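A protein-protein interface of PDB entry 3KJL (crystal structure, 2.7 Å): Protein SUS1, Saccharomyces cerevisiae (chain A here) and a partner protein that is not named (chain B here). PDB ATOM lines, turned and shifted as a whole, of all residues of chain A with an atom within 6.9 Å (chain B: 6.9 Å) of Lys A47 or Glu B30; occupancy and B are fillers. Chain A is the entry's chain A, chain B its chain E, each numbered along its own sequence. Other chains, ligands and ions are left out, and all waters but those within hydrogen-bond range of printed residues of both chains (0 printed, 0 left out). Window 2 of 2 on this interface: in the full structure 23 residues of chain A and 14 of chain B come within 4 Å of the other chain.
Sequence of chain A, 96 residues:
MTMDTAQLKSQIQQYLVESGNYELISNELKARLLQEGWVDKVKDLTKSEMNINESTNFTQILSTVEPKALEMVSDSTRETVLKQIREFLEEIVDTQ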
ATOM      1  N   VAL A  42     -24.726  -2.864  11.532  1.00  0.00           N
ATOM      2  CA  VAL A  42     -24.364  -4.031  10.738  1.00  0.00           C
ATOM      3  C   VAL A  42     -25.413  -4.295   9.665  1.00  0.00           C
ATOM      4  O   VAL A  42     -25.079  -4.664   8.542  1.00  0.00           O
ATOM      5  CB  VAL A  42     -24.197  -5.288  11.613  1.00  0.00           C
ATOM      6  CG1 VAL A  42     -24.219  -6.547  10.754  1.00  0.00           C
ATOM      7  CG2 VAL A  42     -22.909  -5.201  12.414  1.00  0.00           C
ATOM      8  N   LYS A  43     -26.681  -4.115  10.019  1.00  0.00           N
ATOM      9  CA  LYS A  43     -27.763  -4.239   9.050  1.00  0.00           C
ATOM     10  C   LYS A  43     -27.540  -3.260   7.903  1.00  0.00           C
ATOM     11  O   LYS A  43     -27.664  -3.618   6.731  1.00  0.00           O
ATOM     12  CB  LYS A  43     -29.116  -3.958   9.707  1.00  0.00           C
ATOM     13  CG  LYS A  43     -29.627  -5.067  10.611  1.00  0.00           C
ATOM     14  CD  LYS A  43     -30.994  -4.708  11.176  1.00  0.00           C
ATOM     15  CE  LYS A  43     -31.628  -5.872  11.922  1.00  0.00           C
ATOM     16  NZ  LYS A  43     -33.011  -5.554  12.380  1.00  0.00           N
ATOM     17  N   ASP A  44     -27.213  -2.021   8.253  1.00  0.00           N
ATOM     18  CA  ASP A  44     -26.962  -0.978   7.267  1.00  0.00           C
ATOM     19  C   ASP A  44     -25.751  -1.324   6.408  1.00  0.00           C
ATOM     20  O   ASP A  44     -25.689  -0.970   5.231  1.00  0.00           O
ATOM     21  CB  ASP A  44     -26.725   0.362   7.966  1.00  0.00           C
ATOM     22  CG  ASP A  44     -27.896   0.787   8.830  1.00  0.00           C
ATOM     23  OD1 ASP A  44     -29.010   0.262   8.623  1.00  0.00           O
ATOM     24  OD2 ASP A  44     -27.703   1.647   9.714  1.00  0.00           O
ATOM     25  N   LEU A  45     -24.786  -2.012   7.010  1.00  0.00           N
ATOM     26  CA  LEU A  45     -23.558  -2.382   6.317  1.00  0.00           C
ATOM     27  C   LEU A  45     -23.811  -3.498   5.308  1.00  0.00           C
ATOM     28  O   LEU A  45     -23.184  -3.543   4.251  1.00  0.00           O
ATOM     29  CB  LEU A  45     -22.491  -2.816   7.326  1.00  0.00           C
ATOM     30  CG  LEU A  45     -21.232  -3.473   6.752  1.00  0.00           C
ATOM     31  CD1 LEU A  45     -20.616  -2.625   5.647  1.00  0.00           C
ATOM     32  CD2 LEU A  45     -20.223  -3.737   7.860  1.00  0.00           C
ATOM     33  N   THR A  46     -24.736  -4.395   5.635  1.00  0.00           N
ATOM     34  CA  THR A  46     -25.058  -5.514   4.758  1.00  0.00           C
ATOM     35  C   THR A  46     -25.722  -5.015   3.481  1.00  0.00           C
ATOM     36  O   THR A  46     -25.397  -5.464   2.383  1.00  0.00           O
ATOM     37  CB  THR A  46     -26.000  -6.519   5.444  1.00  0.00           C
ATOM     38  OG1 THR A  46     -25.342  -7.109   6.571  1.00  0.00           O
ATOM     39  CG2 THR A  46     -26.412  -7.616   4.471  1.00  0.00           C
ATOM     40  N   LYS A  47     -26.658  -4.085   3.639  1.00  0.00           N
ATOM     41  CA  LYS A  47     -27.378  -3.514   2.506  1.00  0.00           C
ATOM     42  C   LYS A  47     -26.461  -2.648   1.647  1.00  0.00           C
ATOM     43  O   LYS A  47     -26.627  -2.575   0.429  1.00  0.00           O
ATOM     44  CB  LYS A  47     -28.567  -2.691   3.003  1.00  0.00           C
ATOM     45  CG  LYS A  47     -29.661  -3.529   3.643  1.00  0.00           C
ATOM     46  CD  LYS A  47     -30.621  -2.682   4.461  1.00  0.00           C
ATOM     47  CE  LYS A  47     -31.641  -3.551   5.179  1.00  0.00           C
ATOM     48  NZ  LYS A  47     -32.539  -2.761   6.065  1.00  0.00           N
ATOM     49  N   SER A  48     -25.497  -1.993   2.284  1.00  0.00           N
ATOM     50  CA  SER A  48     -24.526  -1.174   1.569  1.00  0.00           C
ATOM     51  C   SER A  48     -23.636  -2.043   0.688  1.00  0.00           C
ATOM     52  O   SER A  48     -23.235  -1.633  -0.400  1.00  0.00           O
ATOM     53  CB  SER A  48     -23.666  -0.380   2.554  1.00  0.00           C
ATOM     54  OG  SER A  48     -22.628   0.312   1.881  1.00  0.00           O
ATOM     55  N   GLU A  49     -23.332  -3.247   1.165  1.00  0.00           N
ATOM     56  CA  GLU A  49     -22.491  -4.174   0.417  1.00  0.00           C
ATOM     57  C   GLU A  49     -23.298  -4.895  -0.658  1.00  0.00           C
ATOM     58  O   GLU A  49     -22.741  -5.368  -1.647  1.00  0.00           O
ATOM     59  CB  GLU A  49     -21.839  -5.191   1.357  1.00  0.00           C
ATOM     60  CG  GLU A  49     -20.832  -4.590   2.331  1.00  0.00           C
ATOM     61  CD  GLU A  49     -19.647  -3.945   1.637  1.00  0.00           C
ATOM     62  OE1 GLU A  49     -19.574  -4.004   0.391  1.00  0.00           O
ATOM     63  OE2 GLU A  49     -18.783  -3.379   2.341  1.00  0.00           O
ATOM     64  N   MET A  50     -24.610  -4.979  -0.462  1.00  0.00           N
ATOM     65  CA  MET A  50     -25.491  -5.582  -1.456  1.00  0.00           C
ATOM     66  C   MET A  50     -25.676  -4.629  -2.631  1.00  0.00           C
ATOM     67  O   MET A  50     -25.896  -5.058  -3.764  1.00  0.00           O
ATOM     68  CB  MET A  50     -26.847  -5.922  -0.838  1.00  0.00           C
ATOM     69  CG  MET A  50     -26.828  -7.160   0.038  1.00  0.00           C
ATOM     70  SD  MET A  50     -28.434  -7.484   0.784  1.00  0.00           S
ATOM     71  CE  MET A  50     -28.198  -9.155   1.382  1.00  0.00           C
ATOM     72  N   ASN A  51     -25.587  -3.334  -2.350  1.00  0.00           N
ATOM     73  CA  ASN A  51     -25.680  -2.313  -3.385  1.00  0.00           C
ATOM     74  C   ASN A  51     -24.367  -2.207  -4.151  1.00  0.00           C
ATOM     75  O   ASN A  51     -24.358  -2.051  -5.372  1.00  0.00           O
ATOM     76  CB  ASN A  51     -26.028  -0.960  -2.760  1.00  0.00           C
ATOM     77  CG  ASN A  51     -27.416  -0.939  -2.150  1.00  0.00           C
ATOM     78  OD1 ASN A  51     -28.209  -1.859  -2.351  1.00  0.00           O
ATOM     79  ND2 ASN A  51     -27.717   0.115  -1.400  1.00  0.00           N
ATOM     80  N   ILE A  52     -23.261  -2.299  -3.421  1.00  0.00           N
ATOM     81  CA  ILE A  52     -21.931  -2.210  -4.011  1.00  0.00           C
ATOM     82  C   ILE A  52     -21.655  -3.397  -4.928  1.00  0.00           C
ATOM     83  O   ILE A  52     -21.021  -3.249  -5.972  1.00  0.00           O
ATOM     84  CB  ILE A  52     -20.844  -2.153  -2.918  1.00  0.00           C
ATOM     85  CG1 ILE A  52     -20.807  -0.759  -2.287  1.00  0.00           C
ATOM     86  CG2 ILE A  52     -19.479  -2.504  -3.493  1.00  0.00           C
ATOM     87  CD1 ILE A  52     -19.777  -0.605  -1.197  1.00  0.00           C
ATOM     88  N   THR A  56     -26.325 -10.857  -4.368  1.00  0.00           N
ATOM     89  CA  THR A  56     -26.993 -10.793  -3.073  1.00  0.00           C
ATOM     90  C   THR A  56     -26.795 -12.118  -2.341  1.00  0.00           C
ATOM     91  O   THR A  56     -27.516 -12.434  -1.396  1.00  0.00           O
ATOM     92  CB  THR A  56     -28.500 -10.514  -3.223  1.00  0.00           C
ATOM     93  OG1 THR A  56     -29.115 -11.568  -3.974  1.00  0.00           O
ATOM     94  CG2 THR A  56     -28.728  -9.189  -3.933  1.00  0.00           C
ATOM     95  N   ILE A  61     -21.617 -12.052   0.209  1.00  0.00           N
ATOM     96  CA  ILE A  61     -21.896 -10.875   1.024  1.00  0.00           C
ATOM     97  C   ILE A  61     -21.289 -11.018   2.416  1.00  0.00           C
ATOM     98  O   ILE A  61     -20.942 -10.026   3.057  1.00  0.00           O
ATOM     99  CB  ILE A  61     -23.414 -10.643   1.163  1.00  0.00           C
ATOM    100  CG1 ILE A  61     -24.022 -10.278  -0.193  1.00  0.00           C
ATOM    101  CG2 ILE A  61     -23.700  -9.547   2.180  1.00  0.00           C
ATOM    102  CD1 ILE A  61     -23.582  -8.930  -0.721  1.00  0.00           C
ATOM    103  N   VAL A  65     -18.670  -8.249   4.528  1.00  0.00           N
ATOM    104  CA  VAL A  65     -19.247  -7.621   5.712  1.00  0.00           C
ATOM    105  C   VAL A  65     -18.615  -8.101   7.018  1.00  0.00           C
ATOM    106  O   VAL A  65     -18.453  -7.323   7.956  1.00  0.00           O
ATOM    107  CB  VAL A  65     -20.771  -7.877   5.785  1.00  0.00           C
ATOM    108  CG1 VAL A  65     -21.312  -7.534   7.168  1.00  0.00           C
ATOM    109  CG2 VAL A  65     -21.490  -7.089   4.703  1.00  0.00           C
ATOM    110  N   ASP B  25     -25.967 -14.435  11.435  1.00  0.00           N
ATOM    111  CA  ASP B  25     -27.408 -14.340  11.630  1.00  0.00           C
ATOM    112  C   ASP B  25     -27.953 -13.045  11.037  1.00  0.00           C
ATOM    113  O   ASP B  25     -28.999 -13.037  10.388  1.00  0.00           O
ATOM    114  CB  ASP B  25     -27.746 -14.398  13.123  1.00  0.00           C
ATOM    115  CG  ASP B  25     -27.504 -15.768  13.724  1.00  0.00           C
ATOM    116  OD1 ASP B  25     -27.537 -16.761  12.969  1.00  0.00           O
ATOM    117  OD2 ASP B  25     -27.290 -15.851  14.951  1.00  0.00           O
ATOM    118  N   ILE B  26     -27.232 -11.952  11.263  1.00  0.00           N
ATOM    119  CA  ILE B  26     -27.656 -10.634  10.800  1.00  0.00           C
ATOM    120  C   ILE B  26     -27.563 -10.538   9.282  1.00  0.00           C
ATOM    121  O   ILE B  26     -28.455  -9.995   8.634  1.00  0.00           O
ATOM    122  CB  ILE B  26     -26.800  -9.511  11.431  1.00  0.00           C
ATOM    123  CG1 ILE B  26     -26.908  -9.551  12.958  1.00  0.00           C
ATOM    124  CG2 ILE B  26     -27.236  -8.149  10.912  1.00  0.00           C
ATOM    125  CD1 ILE B  26     -26.000  -8.564  13.669  1.00  0.00           C
ATOM    126  N   VAL B  27     -26.483 -11.071   8.721  1.00  0.00           N
ATOM    127  CA  VAL B  27     -26.260 -11.028   7.280  1.00  0.00           C
ATOM    128  C   VAL B  27     -27.243 -11.930   6.539  1.00  0.00           C
ATOM    129  O   VAL B  27     -27.723 -11.585   5.460  1.00  0.00           O
ATOM    130  CB  VAL B  27     -24.828 -11.469   6.924  1.00  0.00           C
ATOM    131  CG1 VAL B  27     -24.676 -11.626   5.419  1.00  0.00           C
ATOM    132  CG2 VAL B  27     -23.818 -10.470   7.464  1.00  0.00           C
ATOM    133  N   ALA B  28     -27.536 -13.085   7.127  1.00  0.00           N
ATOM    134  CA  ALA B  28     -28.401 -14.071   6.491  1.00  0.00           C
ATOM    135  C   ALA B  28     -29.844 -13.584   6.424  1.00  0.00           C
ATOM    136  O   ALA B  28     -30.559 -13.876   5.467  1.00  0.00           O
ATOM    137  CB  ALA B  28     -28.324 -15.397   7.233  1.00  0.00           C
ATOM    138  N   ARG B  29     -30.271 -12.849   7.444  1.00  0.00           N
ATOM    139  CA  ARG B  29     -31.635 -12.338   7.490  1.00  0.00           C
ATOM    140  C   ARG B  29     -31.866 -11.324   6.374  1.00  0.00           C
ATOM    141  O   ARG B  29     -32.939 -11.282   5.774  1.00  0.00           O
ATOM    142  CB  ARG B  29     -31.927 -11.692   8.845  1.00  0.00           C
ATOM    143  CG  ARG B  29     -33.369 -11.240   9.001  1.00  0.00           C
ATOM    144  CD  ARG B  29     -33.646 -10.689  10.392  1.00  0.00           C
ATOM    145  NE  ARG B  29     -33.255 -11.624  11.446  1.00  0.00           N
ATOM    146  CZ  ARG B  29     -32.307 -11.392  12.351  1.00  0.00           C
ATOM    147  NH1 ARG B  29     -31.637 -10.245  12.354  1.00  0.00           N
ATOM    148  NH2 ARG B  29     -32.030 -12.312  13.265  1.00  0.00           N
ATOM    149  N   GLU B  30     -30.852 -10.510   6.099  1.00  0.00           N
ATOM    150  CA  GLU B  30     -30.948  -9.502   5.051  1.00  0.00           C
ATOM    151  C   GLU B  30     -30.794 -10.138   3.673  1.00  0.00           C
ATOM    152  O   GLU B  30     -31.152  -9.539   2.658  1.00  0.00           O
ATOM    153  CB  GLU B  30     -29.885  -8.420   5.247  1.00  0.00           C
ATOM    154  CG  GLU B  30     -29.778  -7.914   6.676  1.00  0.00           C
ATOM    155  CD  GLU B  30     -31.123  -7.543   7.268  1.00  0.00           C
ATOM    156  OE1 GLU B  30     -31.973  -7.001   6.530  1.00  0.00           O
ATOM    157  OE2 GLU B  30     -31.331  -7.791   8.475  1.00  0.00           O
ATOM    158  N   THR B  31     -30.263 -11.357   3.645  1.00  0.00           N
ATOM    159  CA  THR B  31     -30.066 -12.087   2.398  1.00  0.00           C
ATOM    160  C   THR B  31     -31.185 -13.095   2.171  1.00  0.00           C
ATOM    161  O   THR B  31     -31.382 -13.998   2.979  1.00  0.00           O
ATOM    162  CB  THR B  31     -28.721 -12.838   2.394  1.00  0.00           C
ATOM    163  OG1 THR B  31     -27.648 -11.906   2.209  1.00  0.00           O
ATOM    164  CG2 THR B  31     -28.684 -13.875   1.278  1.00  0.00           C
ATOM    165  N   THR B  32     -31.898 -12.922   1.060  1.00  0.00           N
ATOM    166  CA  THR B  32     -32.983 -13.811   0.625  1.00  0.00           C
ATOM    167  C   THR B  32     -34.316 -13.070   0.629  1.00  0.00           C
ATOM    168  O   THR B  32     -34.361 -11.847   0.489  1.00  0.00           O
ATOM    169  CB  THR B  32     -33.124 -15.095   1.485  1.00  0.00           C
ATOM    170  OG1 THR B  32     -33.800 -16.107   0.726  1.00  0.00           O
ATOM    171  CG2 THR B  32     -33.910 -14.819   2.758  1.00  0.00           C
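OG1 of Thr A46 is in hydrogen-bond range of O of Val A42, 3.2 Å away. The side-chain amide oxygen (OD1) of Asn A51 lies close to the backbone carbonyl oxygen (O) of Lys A47 (3.3 Å). O of Val B27 is in hydrogen-bond range of OG1 of Thr B31, 3.3 Å away.
Hydrophobic or aromatic side chains of chain B within 4 Å of the printed part of chain A: Ile B26 and Val B27. Among the printed residues, no Asp or Glu carboxylate lies within 4 Å of a Lys or Arg side-chain nitrogen of the other chain.
Of the printed residues of chain B, Met A50 touches Glu B30 and Thr B31. Of the printed residues of chain B, Thr A56 touches Thr B31 (3.3 Å). Of the printed residues of chain A, Val B27 touches Thr A46 (3.8 Å), Ile A61 (3.97 Å) and Val A65 (3.9 Å). Of the printed residues of chain A, Glu B30 touches Lys A43, Thr A46, Lys A47 and Met A50. The nearest residue of chain A that does not touch Glu B30 is Val A42 (6.0 Å). The nearest printed residue of chain B that does not touch Lys A43 is Arg B29 (4.4 Å).
Among the printed residues, merely in contact across the chains: Met A50 with Thr B31, Met A50 with Glu B30, Thr A56 with Thr B31, Val A42 with Ile B26, Thr A46 with Glu B30, Lys A47 with Glu B30, Thr A46 with Val B27, Lys A43 with Glu B30, Val A65 with Val B27, Lys A43 with Ile B26 and Ile A61 with Val B27.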
